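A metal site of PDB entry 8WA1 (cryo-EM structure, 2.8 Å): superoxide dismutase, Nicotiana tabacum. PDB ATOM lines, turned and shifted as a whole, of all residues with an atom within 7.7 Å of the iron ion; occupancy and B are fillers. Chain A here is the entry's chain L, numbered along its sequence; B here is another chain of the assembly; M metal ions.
O of His 125 lies close to NE1 of Trp 129 (3.3 Å). A ring nitrogen (ND1) of His 125 lies within hydrogen-bond range of the backbone carbonyl oxygen of Gln 121, 2.9 Å away. The backbone carbonyl oxygen (O) of Asp 224 is in hydrogen-bond range of the side-chain hydroxyl (OH) of Tyr 241. ND1 of His 228 lies close to NE2 of His 77, 3.1 Å away. The side-chain carboxylate of Glu 217 of chain B lies within hydrogen-bond range of the backbone NH of His 228 (3.2 Å).
Four residues have an atom within 4 Å of the iron ion: His 73, His 125, Asp 224 and His 228.
The iron ion is bound by the side-chain carboxylate (OD2) of Asp 224, a ring nitrogen (NE2) of His 125, a ring nitrogen (NE2) of His 228 and a ring nitrogen (NE2) of His 73. The iron ion has four donor atoms within binding distance.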
ATOM      1  N   HIS A  73     -18.571  21.966  15.480  1.00  0.00           N
ATOM      2  CA  HIS A  73     -19.647  22.877  15.751  1.00  0.00           C
ATOM      3  C   HIS A  73     -20.816  22.597  14.891  1.00  0.00           C
ATOM      4  O   HIS A  73     -21.884  22.193  15.382  1.00  0.00           O
ATOM      5  CB  HIS A  73     -19.114  24.282  15.469  1.00  0.00           C
ATOM      6  CG  HIS A  73     -20.125  25.376  15.565  1.00  0.00           C
ATOM      7  ND1 HIS A  73     -19.946  26.604  14.960  1.00  0.00           N
ATOM      8  CD2 HIS A  73     -21.324  25.457  16.192  1.00  0.00           C
ATOM      9  CE1 HIS A  73     -20.984  27.377  15.202  1.00  0.00           C
ATOM     10  NE2 HIS A  73     -21.835  26.701  15.951  1.00  0.00           N
ATOM     11  N   TRP A  74     -20.575  22.518  13.605  1.00  0.00           N
ATOM     12  CA  TRP A  74     -21.718  22.449  12.737  1.00  0.00           C
ATOM     13  C   TRP A  74     -22.472  21.230  12.986  1.00  0.00           C
ATOM     14  O   TRP A  74     -23.632  21.289  13.379  1.00  0.00           O
ATOM     15  CB  TRP A  74     -21.260  22.422  11.281  1.00  0.00           C
ATOM     16  CG  TRP A  74     -22.368  22.127  10.291  1.00  0.00           C
ATOM     17  CD1 TRP A  74     -23.348  22.976   9.886  1.00  0.00           C
ATOM     18  CD2 TRP A  74     -22.604  20.895   9.582  1.00  0.00           C
ATOM     19  NE1 TRP A  74     -24.185  22.375   8.985  1.00  0.00           N
ATOM     20  CE2 TRP A  74     -23.744  21.093   8.777  1.00  0.00           C
ATOM     21  CE3 TRP A  74     -21.963  19.657   9.563  1.00  0.00           C
ATOM     22  CZ2 TRP A  74     -24.259  20.086   7.960  1.00  0.00           C
ATOM     23  CZ3 TRP A  74     -22.471  18.663   8.744  1.00  0.00           C
ATOM     24  CH2 TRP A  74     -23.605  18.893   7.953  1.00  0.00           C
ATOM     25  N   HIS A  77     -24.257  20.905  16.509  1.00  0.00           N
ATOM     26  CA  HIS A  77     -25.355  21.776  16.809  1.00  0.00           C
ATOM     27  C   HIS A  77     -26.523  21.567  15.903  1.00  0.00           C
ATOM     28  O   HIS A  77     -27.649  21.379  16.358  1.00  0.00           O
ATOM     29  CB  HIS A  77     -24.882  23.213  16.927  1.00  0.00           C
ATOM     30  CG  HIS A  77     -24.023  23.440  18.127  1.00  0.00           C
ATOM     31  ND1 HIS A  77     -24.540  23.707  19.373  1.00  0.00           N
ATOM     32  CD2 HIS A  77     -22.674  23.354  18.286  1.00  0.00           C
ATOM     33  CE1 HIS A  77     -23.554  23.809  20.248  1.00  0.00           C
ATOM     34  NE2 HIS A  77     -22.413  23.603  19.614  1.00  0.00           N
ATOM     35  N   HIS A  78     -26.252  21.467  14.623  1.00  0.00           N
ATOM     36  CA  HIS A  78     -27.377  21.391  13.730  1.00  0.00           C
ATOM     37  C   HIS A  78     -28.124  20.133  13.961  1.00  0.00           C
ATOM     38  O   HIS A  78     -29.344  20.143  14.055  1.00  0.00           O
ATOM     39  CB  HIS A  78     -26.919  21.489  12.297  1.00  0.00           C
ATOM     40  CG  HIS A  78     -27.266  22.793  11.657  1.00  0.00           C
ATOM     41  ND1 HIS A  78     -28.331  22.934  10.796  1.00  0.00           N
ATOM     42  CD2 HIS A  78     -26.722  24.026  11.778  1.00  0.00           C
ATOM     43  CE1 HIS A  78     -28.416  24.190  10.397  1.00  0.00           C
ATOM     44  NE2 HIS A  78     -27.451  24.878  10.988  1.00  0.00           N
ATOM     45  N   TYR A  81     -30.214  20.210  17.121  1.00  0.00           N
ATOM     46  CA  TYR A  81     -31.384  21.037  17.116  1.00  0.00           C
ATOM     47  C   TYR A  81     -32.439  20.387  16.264  1.00  0.00           C
ATOM     48  O   TYR A  81     -33.554  20.199  16.711  1.00  0.00           O
ATOM     49  CB  TYR A  81     -31.072  22.439  16.602  1.00  0.00           C
ATOM     50  CG  TYR A  81     -30.096  23.202  17.458  1.00  0.00           C
ATOM     51  CD1 TYR A  81     -30.158  23.144  18.845  1.00  0.00           C
ATOM     52  CD2 TYR A  81     -29.115  23.997  16.884  1.00  0.00           C
ATOM     53  CE1 TYR A  81     -29.263  23.845  19.620  1.00  0.00           C
ATOM     54  CE2 TYR A  81     -28.217  24.694  17.649  1.00  0.00           C
ATOM     55  CZ  TYR A  81     -28.293  24.617  19.028  1.00  0.00           C
ATOM     56  OH  TYR A  81     -27.400  25.327  19.799  1.00  0.00           O
ATOM     57  N   GLN A 121     -32.408  28.280  17.049  1.00  0.00           N
ATOM     58  CA  GLN A 121     -30.982  28.061  17.002  1.00  0.00           C
ATOM     59  C   GLN A 121     -30.552  27.471  15.685  1.00  0.00           C
ATOM     60  O   GLN A 121     -29.559  27.907  15.116  1.00  0.00           O
ATOM     61  CB  GLN A 121     -30.560  27.148  18.137  1.00  0.00           C
ATOM     62  CG  GLN A 121     -30.365  27.869  19.448  1.00  0.00           C
ATOM     63  CD  GLN A 121     -29.133  28.745  19.441  1.00  0.00           C
ATOM     64  OE1 GLN A 121     -28.110  28.389  18.888  1.00  0.00           O
ATOM     65  NE2 GLN A 121     -29.239  29.911  20.068  1.00  0.00           N
ATOM     66  N   ASN A 124     -30.972  30.099  13.086  1.00  0.00           N
ATOM     67  CA  ASN A 124     -29.898  31.065  13.219  1.00  0.00           C
ATOM     68  C   ASN A 124     -28.615  30.473  12.716  1.00  0.00           C
ATOM     69  O   ASN A 124     -27.854  31.127  12.035  1.00  0.00           O
ATOM     70  CB  ASN A 124     -29.724  31.472  14.686  1.00  0.00           C
ATOM     71  CG  ASN A 124     -30.821  32.393  15.178  1.00  0.00           C
ATOM     72  OD1 ASN A 124     -31.772  32.679  14.457  1.00  0.00           O
ATOM     73  ND2 ASN A 124     -30.695  32.854  16.414  1.00  0.00           N
ATOM     74  N   HIS A 125     -28.368  29.215  13.068  1.00  0.00           N
ATOM     75  CA  HIS A 125     -27.125  28.599  12.670  1.00  0.00           C
ATOM     76  C   HIS A 125     -26.997  28.489  11.163  1.00  0.00           C
ATOM     77  O   HIS A 125     -25.956  28.798  10.608  1.00  0.00           O
ATOM     78  CB  HIS A 125     -26.948  27.242  13.342  1.00  0.00           C
ATOM     79  CG  HIS A 125     -26.213  27.301  14.638  1.00  0.00           C
ATOM     80  ND1 HIS A 125     -26.835  27.159  15.860  1.00  0.00           N
ATOM     81  CD2 HIS A 125     -24.898  27.495  14.912  1.00  0.00           C
ATOM     82  CE1 HIS A 125     -25.937  27.257  16.818  1.00  0.00           C
ATOM     83  NE2 HIS A 125     -24.761  27.467  16.273  1.00  0.00           N
ATOM     84  N   PHE A 128     -26.389  31.701   9.726  1.00  0.00           N
ATOM     85  CA  PHE A 128     -25.001  32.042   9.994  1.00  0.00           C
ATOM     86  C   PHE A 128     -24.049  31.399   8.999  1.00  0.00           C
ATOM     87  O   PHE A 128     -23.122  32.045   8.515  1.00  0.00           O
ATOM     88  CB  PHE A 128     -24.656  31.606  11.416  1.00  0.00           C
ATOM     89  CG  PHE A 128     -23.222  31.790  11.784  1.00  0.00           C
ATOM     90  CD1 PHE A 128     -22.684  33.054  11.927  1.00  0.00           C
ATOM     91  CD2 PHE A 128     -22.409  30.695  12.013  1.00  0.00           C
ATOM     92  CE1 PHE A 128     -21.359  33.218  12.280  1.00  0.00           C
ATOM     93  CE2 PHE A 128     -21.078  30.847  12.360  1.00  0.00           C
ATOM     94  CZ  PHE A 128     -20.549  32.113  12.488  1.00  0.00           C
ATOM     95  N   TRP A 129     -24.285  30.141   8.673  1.00  0.00           N
ATOM     96  CA  TRP A 129     -23.432  29.489   7.705  1.00  0.00           C
ATOM     97  C   TRP A 129     -23.599  30.199   6.388  1.00  0.00           C
ATOM     98  O   TRP A 129     -22.612  30.594   5.755  1.00  0.00           O
ATOM     99  CB  TRP A 129     -23.795  28.018   7.534  1.00  0.00           C
ATOM    100  CG  TRP A 129     -23.803  27.226   8.792  1.00  0.00           C
ATOM    101  CD1 TRP A 129     -24.821  26.462   9.256  1.00  0.00           C
ATOM    102  CD2 TRP A 129     -22.745  27.114   9.751  1.00  0.00           C
ATOM    103  NE1 TRP A 129     -24.477  25.881  10.452  1.00  0.00           N
ATOM    104  CE2 TRP A 129     -23.202  26.264  10.770  1.00  0.00           C
ATOM    105  CE3 TRP A 129     -21.457  27.649   9.834  1.00  0.00           C
ATOM    106  CZ2 TRP A 129     -22.422  25.941  11.869  1.00  0.00           C
ATOM    107  CZ3 TRP A 129     -20.684  27.320  10.922  1.00  0.00           C
ATOM    108  CH2 TRP A 129     -21.161  26.476  11.921  1.00  0.00           C
ATOM    109  N   GLY A 173     -25.157  34.628  22.899  1.00  0.00           N
ATOM    110  CA  GLY A 173     -25.949  35.496  22.062  1.00  0.00           C
ATOM    111  C   GLY A 173     -25.608  35.524  20.583  1.00  0.00           C
ATOM    112  O   GLY A 173     -24.600  34.983  20.166  1.00  0.00           O
ATOM    113  N   TRP A 174     -26.476  36.130  19.779  1.00  0.00           N
ATOM    114  CA  TRP A 174     -26.186  36.284  18.363  1.00  0.00           C
ATOM    115  C   TRP A 174     -26.265  37.783  18.125  1.00  0.00           C
ATOM    116  O   TRP A 174     -27.145  38.442  18.663  1.00  0.00           O
ATOM    117  CB  TRP A 174     -27.224  35.568  17.505  1.00  0.00           C
ATOM    118  CG  TRP A 174     -27.295  34.107  17.707  1.00  0.00           C
ATOM    119  CD1 TRP A 174     -27.836  33.451  18.765  1.00  0.00           C
ATOM    120  CD2 TRP A 174     -26.846  33.101  16.802  1.00  0.00           C
ATOM    121  NE1 TRP A 174     -27.732  32.096  18.588  1.00  0.00           N
ATOM    122  CE2 TRP A 174     -27.123  31.854  17.384  1.00  0.00           C
ATOM    123  CE3 TRP A 174     -26.224  33.124  15.544  1.00  0.00           C
ATOM    124  CZ2 TRP A 174     -26.807  30.648  16.770  1.00  0.00           C
ATOM    125  CZ3 TRP A 174     -25.914  31.930  14.935  1.00  0.00           C
ATOM    126  CH2 TRP A 174     -26.196  30.707  15.551  1.00  0.00           C
ATOM    127  N   ASP A 224     -22.271  34.637  15.290  1.00  0.00           N
ATOM    128  CA  ASP A 224     -22.649  33.757  16.365  1.00  0.00           C
ATOM    129  C   ASP A 224     -21.682  33.995  17.484  1.00  0.00           C
ATOM    130  O   ASP A 224     -20.595  33.429  17.495  1.00  0.00           O
ATOM    131  CB  ASP A 224     -22.545  32.298  15.926  1.00  0.00           C
ATOM    132  CG  ASP A 224     -23.058  31.335  16.965  1.00  0.00           C
ATOM    133  OD1 ASP A 224     -23.864  31.757  17.816  1.00  0.00           O
ATOM    134  OD2 ASP A 224     -22.667  30.157  16.926  1.00  0.00           O
ATOM    135  N   VAL A 225     -22.074  34.837  18.441  1.00  0.00           N
ATOM    136  CA  VAL A 225     -21.225  35.053  19.598  1.00  0.00           C
ATOM    137  C   VAL A 225     -21.555  34.052  20.674  1.00  0.00           C
ATOM    138  O   VAL A 225     -22.140  34.399  21.685  1.00  0.00           O
ATOM    139  CB  VAL A 225     -21.301  36.495  20.106  1.00  0.00           C
ATOM    140  CG1 VAL A 225     -20.027  37.228  19.743  1.00  0.00           C
ATOM    141  CG2 VAL A 225     -22.489  37.219  19.493  1.00  0.00           C
ATOM    142  N   TRP A 226     -21.174  32.814  20.454  1.00  0.00           N
ATOM    143  CA  TRP A 226     -21.400  31.784  21.440  1.00  0.00           C
ATOM    144  C   TRP A 226     -20.026  31.200  21.535  1.00  0.00           C
ATOM    145  O   TRP A 226     -19.241  31.303  20.597  1.00  0.00           O
ATOM    146  CB  TRP A 226     -22.346  30.710  20.942  1.00  0.00           C
ATOM    147  CG  TRP A 226     -23.801  30.966  21.198  1.00  0.00           C
ATOM    148  CD1 TRP A 226     -24.535  32.024  20.776  1.00  0.00           C
ATOM    149  CD2 TRP A 226     -24.702  30.126  21.922  1.00  0.00           C
ATOM    150  NE1 TRP A 226     -25.837  31.911  21.195  1.00  0.00           N
ATOM    151  CE2 TRP A 226     -25.969  30.741  21.894  1.00  0.00           C
ATOM    152  CE3 TRP A 226     -24.564  28.900  22.581  1.00  0.00           C
ATOM    153  CZ2 TRP A 226     -27.078  30.195  22.509  1.00  0.00           C
ATOM    154  CZ3 TRP A 226     -25.673  28.355  23.195  1.00  0.00           C
ATOM    155  CH2 TRP A 226     -26.915  28.994  23.155  1.00  0.00           C
ATOM    156  N   GLU A 227     -19.727  30.577  22.643  1.00  0.00           N
ATOM    157  CA  GLU A 227     -18.380  30.067  22.847  1.00  0.00           C
ATOM    158  C   GLU A 227     -17.993  29.012  21.851  1.00  0.00           C
ATOM    159  O   GLU A 227     -16.867  28.983  21.394  1.00  0.00           O
ATOM    160  CB  GLU A 227     -18.212  29.554  24.274  1.00  0.00           C
ATOM    161  CG  GLU A 227     -17.670  30.591  25.243  1.00  0.00           C
ATOM    162  CD  GLU A 227     -18.441  30.619  26.547  1.00  0.00           C
ATOM    163  OE1 GLU A 227     -19.575  30.111  26.591  1.00  0.00           O
ATOM    164  OE2 GLU A 227     -17.908  31.176  27.545  1.00  0.00           O
ATOM    165  N   HIS A 228     -18.929  28.174  21.441  1.00  0.00           N
ATOM    166  CA  HIS A 228     -18.548  27.074  20.580  1.00  0.00           C
ATOM    167  C   HIS A 228     -17.872  27.560  19.324  1.00  0.00           C
ATOM    168  O   HIS A 228     -16.952  26.915  18.837  1.00  0.00           O
ATOM    169  CB  HIS A 228     -19.726  26.150  20.257  1.00  0.00           C
ATOM    170  CG  HIS A 228     -20.981  26.853  19.828  1.00  0.00           C
ATOM    171  ND1 HIS A 228     -22.207  26.592  20.397  1.00  0.00           N
ATOM    172  CD2 HIS A 228     -21.210  27.763  18.853  1.00  0.00           C
ATOM    173  CE1 HIS A 228     -23.129  27.322  19.809  1.00  0.00           C
ATOM    174  NE2 HIS A 228     -22.557  28.040  18.871  1.00  0.00           N
ATOM    175  N   ALA A 229     -18.296  28.703  18.814  1.00  0.00           N
ATOM    176  CA  ALA A 229     -17.750  29.184  17.564  1.00  0.00           C
ATOM    177  C   ALA A 229     -16.259  29.441  17.617  1.00  0.00           C
ATOM    178  O   ALA A 229     -15.543  29.089  16.681  1.00  0.00           O
ATOM    179  CB  ALA A 229     -18.473  30.436  17.134  1.00  0.00           C
ATOM    180  N   TYR A 241     -11.875  36.733  17.198  1.00  0.00           N
ATOM    181  CA  TYR A 241     -12.840  36.088  16.317  1.00  0.00           C
ATOM    182  C   TYR A 241     -13.740  37.111  15.680  1.00  0.00           C
ATOM    183  O   TYR A 241     -14.049  37.027  14.501  1.00  0.00           O
ATOM    184  CB  TYR A 241     -13.660  35.069  17.116  1.00  0.00           C
ATOM    185  CG  TYR A 241     -15.039  34.763  16.586  1.00  0.00           C
ATOM    186  CD1 TYR A 241     -15.219  33.902  15.514  1.00  0.00           C
ATOM    187  CD2 TYR A 241     -16.166  35.302  17.188  1.00  0.00           C
ATOM    188  CE1 TYR A 241     -16.488  33.623  15.042  1.00  0.00           C
ATOM    189  CE2 TYR A 241     -17.425  35.027  16.717  1.00  0.00           C
ATOM    190  CZ  TYR A 241     -17.590  34.182  15.645  1.00  0.00           C
ATOM    191  OH  TYR A 241     -18.847  33.898  15.178  1.00  0.00           O
ATOM    192  N   GLU B 217     -20.070  27.611  28.887  1.00  0.00           N
ATOM    193  CA  GLU B 217     -19.325  26.678  28.059  1.00  0.00           C
ATOM    194  C   GLU B 217     -17.831  26.739  28.235  1.00  0.00           C
ATOM    195  O   GLU B 217     -17.157  25.729  28.060  1.00  0.00           O
ATOM    196  CB  GLU B 217     -19.680  26.860  26.588  1.00  0.00           C
ATOM    197  CG  GLU B 217     -21.170  26.808  26.301  1.00  0.00           C
ATOM    198  CD  GLU B 217     -21.489  26.957  24.831  1.00  0.00           C
ATOM    199  OE1 GLU B 217     -20.559  27.131  24.024  1.00  0.00           O
ATOM    200  OE2 GLU B 217     -22.691  26.892  24.482  1.00  0.00           O
ATOM    201  N   TYR B 221     -15.855  23.173  27.330  1.00  0.00           N
ATOM    202  CA  TYR B 221     -15.609  22.868  25.914  1.00  0.00           C
ATOM    203  C   TYR B 221     -14.258  22.255  25.572  1.00  0.00           C
ATOM    204  O   TYR B 221     -14.197  21.335  24.760  1.00  0.00           O
ATOM    205  CB  TYR B 221     -15.847  24.106  25.045  1.00  0.00           C
ATOM    206  CG  TYR B 221     -16.671  23.832  23.816  1.00  0.00           C
ATOM    207  CD1 TYR B 221     -16.093  23.282  22.685  1.00  0.00           C
ATOM    208  CD2 TYR B 221     -18.018  24.133  23.783  1.00  0.00           C
ATOM    209  CE1 TYR B 221     -16.846  23.031  21.559  1.00  0.00           C
ATOM    210  CE2 TYR B 221     -18.783  23.881  22.664  1.00  0.00           C
ATOM    211  CZ  TYR B 221     -18.184  23.323  21.553  1.00  0.00           C
ATOM    212  OH  TYR B 221     -18.949  23.072  20.434  1.00  0.00           O
HETATM  213 FE    FE M   1     -23.224  28.364  17.047  1.00  0.00          FE
